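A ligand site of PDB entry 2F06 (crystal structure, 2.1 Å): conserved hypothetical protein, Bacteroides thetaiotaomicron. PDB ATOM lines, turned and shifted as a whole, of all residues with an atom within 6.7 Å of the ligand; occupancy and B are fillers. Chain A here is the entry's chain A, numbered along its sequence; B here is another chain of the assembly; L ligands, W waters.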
ATOM      1  N   CYS A  79      30.790 -31.931   1.344  1.00  0.00           N
ATOM      2  CA  CYS A  79      31.303 -32.217  -0.001  1.00  0.00           C
ATOM      3  C   CYS A  79      32.262 -31.130  -0.438  1.00  0.00           C
ATOM      4  O   CYS A  79      32.414 -30.145   0.252  1.00  0.00           O
ATOM      5  CB  CYS A  79      30.158 -32.363  -1.006  1.00  0.00           C
ATOM      6  SG  CYS A  79      29.109 -30.917  -1.080  1.00  0.00           S
ATOM      7  N   PRO A  80      32.961 -31.330  -1.535  1.00  0.00           N
ATOM      8  CA  PRO A  80      33.789 -30.195  -2.002  1.00  0.00           C
ATOM      9  C   PRO A  80      33.019 -28.886  -2.318  1.00  0.00           C
ATOM     10  O   PRO A  80      31.846 -28.911  -2.744  1.00  0.00           O
ATOM     11  CB  PRO A  80      34.541 -30.785  -3.213  1.00  0.00           C
ATOM     12  CG  PRO A  80      34.670 -32.257  -2.838  1.00  0.00           C
ATOM     13  CD  PRO A  80      33.292 -32.570  -2.284  1.00  0.00           C
ATOM     14  N   ASN A  81      33.699 -27.765  -2.055  1.00  0.00           N
ATOM     15  CA  ASN A  81      33.125 -26.458  -2.351  1.00  0.00           C
ATOM     16  C   ASN A  81      33.489 -26.088  -3.762  1.00  0.00           C
ATOM     17  O   ASN A  81      34.197 -25.103  -3.999  1.00  0.00           O
ATOM     18  CB  ASN A  81      33.565 -25.362  -1.349  1.00  0.00           C
ATOM     19  CG  ASN A  81      32.843 -24.036  -1.601  1.00  0.00           C
ATOM     20  OD1 ASN A  81      31.737 -24.023  -2.113  1.00  0.00           O
ATOM     21  ND2 ASN A  81      33.491 -22.906  -1.253  1.00  0.00           N
ATOM     22  N   VAL A  82      32.963 -26.863  -4.706  1.00  0.00           N
ATOM     23  CA  VAL A  82      33.160 -26.621  -6.139  1.00  0.00           C
ATOM     24  C   VAL A  82      31.818 -26.827  -6.847  1.00  0.00           C
ATOM     25  O   VAL A  82      30.955 -27.479  -6.286  1.00  0.00           O
ATOM     26  CB  VAL A  82      34.377 -27.412  -6.776  1.00  0.00           C
ATOM     27  CG1 VAL A  82      35.678 -27.221  -5.970  1.00  0.00           C
ATOM     28  CG2 VAL A  82      34.088 -28.924  -7.038  1.00  0.00           C
ATOM     29  N   PRO A  83      31.610 -26.185  -8.031  1.00  0.00           N
ATOM     30  CA  PRO A  83      30.402 -26.374  -8.818  1.00  0.00           C
ATOM     31  C   PRO A  83      30.095 -27.837  -9.110  1.00  0.00           C
ATOM     32  O   PRO A  83      31.009 -28.610  -9.461  1.00  0.00           O
ATOM     33  CB  PRO A  83      30.748 -25.616 -10.111  1.00  0.00           C
ATOM     34  CG  PRO A  83      31.472 -24.416  -9.540  1.00  0.00           C
ATOM     35  CD  PRO A  83      32.455 -25.152  -8.669  1.00  0.00           C
ATOM     36  N   GLY A  84      28.823 -28.215  -8.938  1.00  0.00           N
ATOM     37  CA  GLY A  84      28.371 -29.568  -9.298  1.00  0.00           C
ATOM     38  C   GLY A  84      28.567 -30.626  -8.229  1.00  0.00           C
ATOM     39  O   GLY A  84      28.216 -31.800  -8.429  1.00  0.00           O
ATOM     40  N   ALA A  85      29.133 -30.209  -7.091  1.00  0.00           N
ATOM     41  CA  ALA A  85      29.537 -31.133  -6.071  1.00  0.00           C
ATOM     42  C   ALA A  85      28.284 -31.625  -5.374  1.00  0.00           C
ATOM     43  O   ALA A  85      28.101 -32.826  -5.238  1.00  0.00           O
ATOM     44  CB  ALA A  85      30.457 -30.447  -5.117  1.00  0.00           C
ATOM     45  N   LEU A  86      27.417 -30.695  -4.972  1.00  0.00           N
ATOM     46  CA  LEU A  86      26.124 -31.048  -4.373  1.00  0.00           C
ATOM     47  C   LEU A  86      25.232 -31.807  -5.362  1.00  0.00           C
ATOM     48  O   LEU A  86      24.556 -32.752  -4.971  1.00  0.00           O
ATOM     49  CB  LEU A  86      25.390 -29.792  -3.860  1.00  0.00           C
ATOM     50  CG  LEU A  86      24.059 -30.011  -3.124  1.00  0.00           C
ATOM     51  CD1 LEU A  86      24.152 -31.048  -1.949  1.00  0.00           C
ATOM     52  CD2 LEU A  86      23.517 -28.677  -2.650  1.00  0.00           C
ATOM     53  N   ALA A  87      25.242 -31.368  -6.627  1.00  0.00           N
ATOM     54  CA  ALA A  87      24.586 -31.994  -7.754  1.00  0.00           C
ATOM     55  C   ALA A  87      24.831 -33.491  -7.832  1.00  0.00           C
ATOM     56  O   ALA A  87      23.923 -34.231  -8.204  1.00  0.00           O
ATOM     57  CB  ALA A  87      25.070 -31.355  -9.092  1.00  0.00           C
ATOM     58  N   MET A 103      16.675 -29.062   2.988  1.00  0.00           N
ATOM     59  CA  MET A 103      18.111 -29.038   3.311  1.00  0.00           C
ATOM     60  C   MET A 103      18.494 -27.609   3.502  1.00  0.00           C
ATOM     61  O   MET A 103      17.764 -26.743   3.045  1.00  0.00           O
ATOM     62  CB  MET A 103      18.955 -29.673   2.171  1.00  0.00           C
ATOM     63  CG  MET A 103      19.327 -28.729   1.015  1.00  0.00           C
ATOM     64  SD  MET A 103      20.218 -29.842  -0.326  1.00  0.00           S
ATOM     65  CE  MET A 103      19.886 -28.813  -2.010  1.00  0.00           C
ATOM     66  N   TYR A 104      19.612 -27.352   4.170  1.00  0.00           N
ATOM     67  CA  TYR A 104      20.203 -26.052   4.236  1.00  0.00           C
ATOM     68  C   TYR A 104      21.696 -26.276   4.292  1.00  0.00           C
ATOM     69  O   TYR A 104      22.169 -27.342   4.785  1.00  0.00           O
ATOM     70  CB  TYR A 104      19.657 -25.210   5.457  1.00  0.00           C
ATOM     71  CG  TYR A 104      19.490 -25.922   6.799  1.00  0.00           C
ATOM     72  CD1 TYR A 104      18.381 -26.775   7.035  1.00  0.00           C
ATOM     73  CD2 TYR A 104      20.371 -25.693   7.869  1.00  0.00           C
ATOM     74  CE1 TYR A 104      18.190 -27.373   8.307  1.00  0.00           C
ATOM     75  CE2 TYR A 104      20.211 -26.356   9.135  1.00  0.00           C
ATOM     76  CZ  TYR A 104      19.098 -27.168   9.335  1.00  0.00           C
ATOM     77  OH  TYR A 104      18.876 -27.795  10.550  1.00  0.00           O
ATOM     78  N   SER A 105      22.472 -25.309   3.780  1.00  0.00           N
ATOM     79  CA  SER A 105      23.892 -25.487   3.685  1.00  0.00           C
ATOM     80  C   SER A 105      24.670 -24.239   3.357  1.00  0.00           C
ATOM     81  O   SER A 105      24.109 -23.296   2.800  1.00  0.00           O
ATOM     82  CB  SER A 105      24.169 -26.534   2.606  1.00  0.00           C
ATOM     83  OG  SER A 105      23.530 -26.146   1.415  1.00  0.00           O
ATOM     84  N   PHE A 106      25.939 -24.195   3.804  1.00  0.00           N
ATOM     85  CA  PHE A 106      26.843 -23.065   3.546  1.00  0.00           C
ATOM     86  C   PHE A 106      28.157 -23.683   3.083  1.00  0.00           C
ATOM     87  O   PHE A 106      28.542 -24.763   3.553  1.00  0.00           O
ATOM     88  CB  PHE A 106      27.151 -22.190   4.783  1.00  0.00           C
ATOM     89  CG  PHE A 106      26.363 -20.891   4.880  1.00  0.00           C
ATOM     90  CD1 PHE A 106      25.015 -20.877   5.290  1.00  0.00           C
ATOM     91  CD2 PHE A 106      26.979 -19.676   4.567  1.00  0.00           C
ATOM     92  CE1 PHE A 106      24.289 -19.662   5.384  1.00  0.00           C
ATOM     93  CE2 PHE A 106      26.296 -18.471   4.625  1.00  0.00           C
ATOM     94  CZ  PHE A 106      24.929 -18.456   5.056  1.00  0.00           C
ATOM     95  N   ALA A 107      28.878 -22.967   2.237  1.00  0.00           N
ATOM     96  CA  ALA A 107      30.282 -23.243   1.988  1.00  0.00           C
ATOM     97  C   ALA A 107      31.141 -22.842   3.199  1.00  0.00           C
ATOM     98  O   ALA A 107      30.998 -21.753   3.728  1.00  0.00           O
ATOM     99  CB  ALA A 107      30.761 -22.493   0.724  1.00  0.00           C
ATOM    100  N   ASN A 108      32.034 -23.746   3.590  1.00  0.00           N
ATOM    101  CA  ASN A 108      33.007 -23.542   4.660  1.00  0.00           C
ATOM    102  C   ASN A 108      34.419 -23.785   4.065  1.00  0.00           C
ATOM    103  O   ASN A 108      34.933 -24.909   3.978  1.00  0.00           O
ATOM    104  CB  ASN A 108      32.627 -24.421   5.881  1.00  0.00           C
ATOM    105  CG  ASN A 108      33.789 -24.711   6.820  1.00  0.00           C
ATOM    106  OD1 ASN A 108      34.450 -25.750   6.708  1.00  0.00           O
ATOM    107  ND2 ASN A 108      34.041 -23.812   7.757  1.00  0.00           N
ATOM    108  N   VAL A 111      35.293 -26.901   1.765  1.00  0.00           N
ATOM    109  CA  VAL A 111      34.181 -27.862   1.716  1.00  0.00           C
ATOM    110  C   VAL A 111      32.866 -27.131   1.924  1.00  0.00           C
ATOM    111  O   VAL A 111      32.818 -25.922   2.076  1.00  0.00           O
ATOM    112  CB  VAL A 111      34.315 -29.007   2.771  1.00  0.00           C
ATOM    113  CG1 VAL A 111      35.583 -29.853   2.556  1.00  0.00           C
ATOM    114  CG2 VAL A 111      34.261 -28.442   4.158  1.00  0.00           C
ATOM    115  N   ALA A 112      31.774 -27.868   1.953  1.00  0.00           N
ATOM    116  CA  ALA A 112      30.485 -27.290   2.208  1.00  0.00           C
ATOM    117  C   ALA A 112      29.790 -28.269   3.120  1.00  0.00           C
ATOM    118  O   ALA A 112      29.965 -29.459   2.981  1.00  0.00           O
ATOM    119  CB  ALA A 112      29.721 -27.150   0.918  1.00  0.00           C
ATOM    120  N   ASN A 113      29.079 -27.762   4.104  1.00  0.00           N
ATOM    121  CA  ASN A 113      28.353 -28.562   5.070  1.00  0.00           C
ATOM    122  C   ASN A 113      26.882 -28.531   4.699  1.00  0.00           C
ATOM    123  O   ASN A 113      26.351 -27.472   4.415  1.00  0.00           O
ATOM    124  CB  ASN A 113      28.592 -27.966   6.478  1.00  0.00           C
ATOM    125  CG  ASN A 113      30.013 -28.186   6.934  1.00  0.00           C
ATOM    126  OD1 ASN A 113      30.764 -27.230   7.208  1.00  0.00           O
ATOM    127  ND2 ASN A 113      30.436 -29.424   6.964  1.00  0.00           N
ATOM    128  N   VAL A 114      26.240 -29.683   4.680  1.00  0.00           N
ATOM    129  CA  VAL A 114      24.859 -29.746   4.246  1.00  0.00           C
ATOM    130  C   VAL A 114      24.083 -30.532   5.280  1.00  0.00           C
ATOM    131  O   VAL A 114      24.486 -31.626   5.631  1.00  0.00           O
ATOM    132  CB  VAL A 114      24.679 -30.444   2.833  1.00  0.00           C
ATOM    133  CG1 VAL A 114      23.239 -30.187   2.308  1.00  0.00           C
ATOM    134  CG2 VAL A 114      25.759 -29.945   1.836  1.00  0.00           C
ATOM    135  N   THR B  24      20.372 -28.047  -9.715  1.00  0.00           N
ATOM    136  CA  THR B  24      21.795 -28.027  -9.345  1.00  0.00           C
ATOM    137  C   THR B  24      22.671 -28.419 -10.533  1.00  0.00           C
ATOM    138  O   THR B  24      23.826 -27.955 -10.627  1.00  0.00           O
ATOM    139  CB  THR B  24      22.135 -28.931  -8.132  1.00  0.00           C
ATOM    140  OG1 THR B  24      21.661 -30.263  -8.378  1.00  0.00           O
ATOM    141  CG2 THR B  24      21.512 -28.305  -6.801  1.00  0.00           C
ATOM    142  N   ALA B  28      25.671 -26.242 -12.098  1.00  0.00           N
ATOM    143  CA  ALA B  28      26.966 -26.909 -12.311  1.00  0.00           C
ATOM    144  C   ALA B  28      27.491 -26.709 -13.722  1.00  0.00           C
ATOM    145  O   ALA B  28      28.719 -26.560 -13.937  1.00  0.00           O
ATOM    146  CB  ALA B  28      26.845 -28.409 -12.073  1.00  0.00           C
ATOM    147  N   ILE B  32      28.795 -22.417 -11.911  1.00  0.00           N
ATOM    148  CA  ILE B  32      28.285 -21.526 -10.914  1.00  0.00           C
ATOM    149  C   ILE B  32      28.338 -22.272  -9.625  1.00  0.00           C
ATOM    150  O   ILE B  32      27.777 -23.365  -9.484  1.00  0.00           O
ATOM    151  CB  ILE B  32      26.911 -20.922 -11.278  1.00  0.00           C
ATOM    152  CG1 ILE B  32      27.034 -19.931 -12.439  1.00  0.00           C
ATOM    153  CG2 ILE B  32      26.343 -20.028 -10.101  1.00  0.00           C
ATOM    154  CD1 ILE B  32      25.717 -19.498 -13.116  1.00  0.00           C
ATOM    155  N   ASN B  33      29.085 -21.697  -8.680  1.00  0.00           N
ATOM    156  CA  ASN B  33      29.176 -22.235  -7.312  1.00  0.00           C
ATOM    157  C   ASN B  33      28.025 -21.761  -6.421  1.00  0.00           C
ATOM    158  O   ASN B  33      27.644 -20.558  -6.379  1.00  0.00           O
ATOM    159  CB  ASN B  33      30.528 -21.826  -6.630  1.00  0.00           C
ATOM    160  CG  ASN B  33      30.912 -22.741  -5.454  1.00  0.00           C
ATOM    161  OD1 ASN B  33      30.941 -23.959  -5.602  1.00  0.00           O
ATOM    162  ND2 ASN B  33      31.177 -22.156  -4.293  1.00  0.00           N
ATOM    163  N   LEU B  34      27.545 -22.689  -5.612  1.00  0.00           N
ATOM    164  CA  LEU B  34      26.576 -22.396  -4.572  1.00  0.00           C
ATOM    165  C   LEU B  34      27.316 -22.045  -3.285  1.00  0.00           C
ATOM    166  O   LEU B  34      28.143 -22.788  -2.833  1.00  0.00           O
ATOM    167  CB  LEU B  34      25.700 -23.637  -4.386  1.00  0.00           C
ATOM    168  CG  LEU B  34      24.788 -24.078  -5.567  1.00  0.00           C
ATOM    169  CD1 LEU B  34      24.268 -25.499  -5.332  1.00  0.00           C
ATOM    170  CD2 LEU B  34      23.588 -23.173  -5.672  1.00  0.00           C
ATOM    171  N   SER B  35      27.012 -20.914  -2.668  1.00  0.00           N
ATOM    172  CA  SER B  35      27.627 -20.475  -1.398  1.00  0.00           C
ATOM    173  C   SER B  35      26.851 -20.861  -0.181  1.00  0.00           C
ATOM    174  O   SER B  35      27.400 -21.142   0.868  1.00  0.00           O
ATOM    175  CB  SER B  35      27.705 -18.953  -1.397  1.00  0.00           C
ATOM    176  OG  SER B  35      28.836 -18.618  -2.118  1.00  0.00           O
ATOM    177  N   ALA B  36      25.548 -20.795  -0.347  1.00  0.00           N
ATOM    178  CA  ALA B  36      24.582 -20.907   0.747  1.00  0.00           C
ATOM    179  C   ALA B  36      23.234 -21.185   0.117  1.00  0.00           C
ATOM    180  O   ALA B  36      22.818 -20.519  -0.857  1.00  0.00           O
ATOM    181  CB  ALA B  36      24.491 -19.625   1.563  1.00  0.00           C
ATOM    182  N   LEU B  37      22.543 -22.142   0.689  1.00  0.00           N
ATOM    183  CA  LEU B  37      21.198 -22.346   0.271  1.00  0.00           C
ATOM    184  C   LEU B  37      20.340 -22.871   1.412  1.00  0.00           C
ATOM    185  O   LEU B  37      20.861 -23.306   2.456  1.00  0.00           O
ATOM    186  CB  LEU B  37      21.150 -23.241  -0.952  1.00  0.00           C
ATOM    187  CG  LEU B  37      21.769 -24.591  -0.825  1.00  0.00           C
ATOM    188  CD1 LEU B  37      21.013 -25.357   0.305  1.00  0.00           C
ATOM    189  CD2 LEU B  37      21.699 -25.273  -2.212  1.00  0.00           C
ATOM    190  N   ILE B  51      22.188 -18.526  -2.430  1.00  0.00           N
ATOM    191  CA  ILE B  51      23.306 -17.611  -2.703  1.00  0.00           C
ATOM    192  C   ILE B  51      24.297 -18.293  -3.661  1.00  0.00           C
ATOM    193  O   ILE B  51      24.851 -19.333  -3.327  1.00  0.00           O
ATOM    194  CB  ILE B  51      24.005 -17.099  -1.399  1.00  0.00           C
ATOM    195  CG1 ILE B  51      22.964 -16.449  -0.485  1.00  0.00           C
ATOM    196  CG2 ILE B  51      25.149 -16.136  -1.767  1.00  0.00           C
ATOM    197  CD1 ILE B  51      22.551 -15.037  -0.851  1.00  0.00           C
ATOM    198  N   LEU B 144      31.905 -17.418  -1.121  1.00  0.00           N
ATOM    199  CA  LEU B 144      32.224 -18.163   0.088  1.00  0.00           C
ATOM    200  C   LEU B 144      32.774 -19.574  -0.245  1.00  0.00           C
ATOM    201  O   LEU B 144      33.585 -20.199   0.485  1.00  0.00           O
ATOM    202  CB  LEU B 144      31.008 -18.244   1.011  1.00  0.00           C
ATOM    203  CG  LEU B 144      30.558 -17.006   1.784  1.00  0.00           C
ATOM    204  CD1 LEU B 144      29.274 -17.333   2.496  1.00  0.00           C
ATOM    205  CD2 LEU B 144      31.607 -16.710   2.842  1.00  0.00           C
ATOM    206  OXT LEU B 144      32.401 -20.131  -1.305  1.00  0.00           O
HETATM  207  N1  LIG L   1      29.808 -25.074  -3.612  1.00  0.00           N
HETATM  208  C1  LIG L   1      29.329 -26.475  -3.876  1.00  0.00           C
HETATM  209  C2  LIG L   1      28.376 -26.699  -5.015  1.00  0.00           C
HETATM  210  O1  LIG L   1      28.171 -25.879  -5.907  1.00  0.00           O
HETATM  211  C3  LIG L   1      28.744 -27.149  -2.621  1.00  0.00           C
HETATM  212  C4  LIG L   1      27.599 -26.425  -1.948  1.00  0.00           C
HETATM  213  N2  LIG L   1      27.774 -25.275  -1.191  1.00  0.00           N
HETATM  214  C5  LIG L   1      26.286 -26.769  -1.789  1.00  0.00           C
HETATM  215  C6  LIG L   1      26.607 -24.910  -0.657  1.00  0.00           C
HETATM  216  N3  LIG L   1      25.692 -25.812  -1.003  1.00  0.00           N
HETATM  217  O2  LIG L   1      27.744 -27.762  -5.050  1.00  0.00           O
HETATM  218  O   HOH W   1      27.289 -25.664  -8.164  1.00  0.00           O
HETATM  219  O   HOH W   2      26.271 -28.727  -7.129  1.00  0.00           O
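OG of Ser 105 is in hydrogen-bond range of N3 of the ligand. The backbone NH of Leu 86 is in hydrogen-bond range of an oxygen (O2) of the ligand (3.0 Å). The backbone carbonyl oxygen of Leu 34 of chain B is in hydrogen-bond range of a nitrogen (N1) of the ligand (2.9 Å). An oxygen (O1) of the ligand lies within hydrogen-bond range of the backbone NH (N) of Leu 34 of chain B (3.3 Å). The backbone NH of Ala 85 sits at hydrogen-bond distance from an oxygen (O2) of the ligand (3.5 Å). A nitrogen (N1) of the ligand sits at hydrogen-bond distance from the side-chain amide oxygen of Asn 33 of chain B (2.5 Å). The side-chain amide oxygen (OD1) of Asn 81 is in hydrogen-bond range of a nitrogen (N1) of the ligand (2.7 Å).
ND2 of Asn 81 sits at hydrogen-bond distance from OXT of Leu 144 of chain B, at 3.0 Å. O of Ser 105 is in hydrogen-bond range of N of Leu 37 of chain B (2.9 Å). The side-chain amide oxygen of Asn 81 lies within hydrogen-bond range of the side-chain amide nitrogen of Asn 33 of chain B, 2.9 Å away. The backbone NH of Ala 112 is in hydrogen-bond range of the backbone carbonyl oxygen of Cys 79, at 2.9 Å.
The backbone carbonyl oxygen (O) of Val 82 lies close to an oxygen (O1) of the ligand (3.2 Å). Residues that only touch the ligand: Ala 112, Pro 80, Pro 83 and Gly 84. Of the 29 residues printed, 11 come within 4 Å of the ligand. The nearest printed residue that does not touch the ligand is Ser 35 of chain B (4.1 Å).
Water W1 lies within hydrogen-bond range of O1 of the ligand (2.4 Å), O of Ile 32 of chain B (2.7 Å) and N of Gly 84 (3.1 Å).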
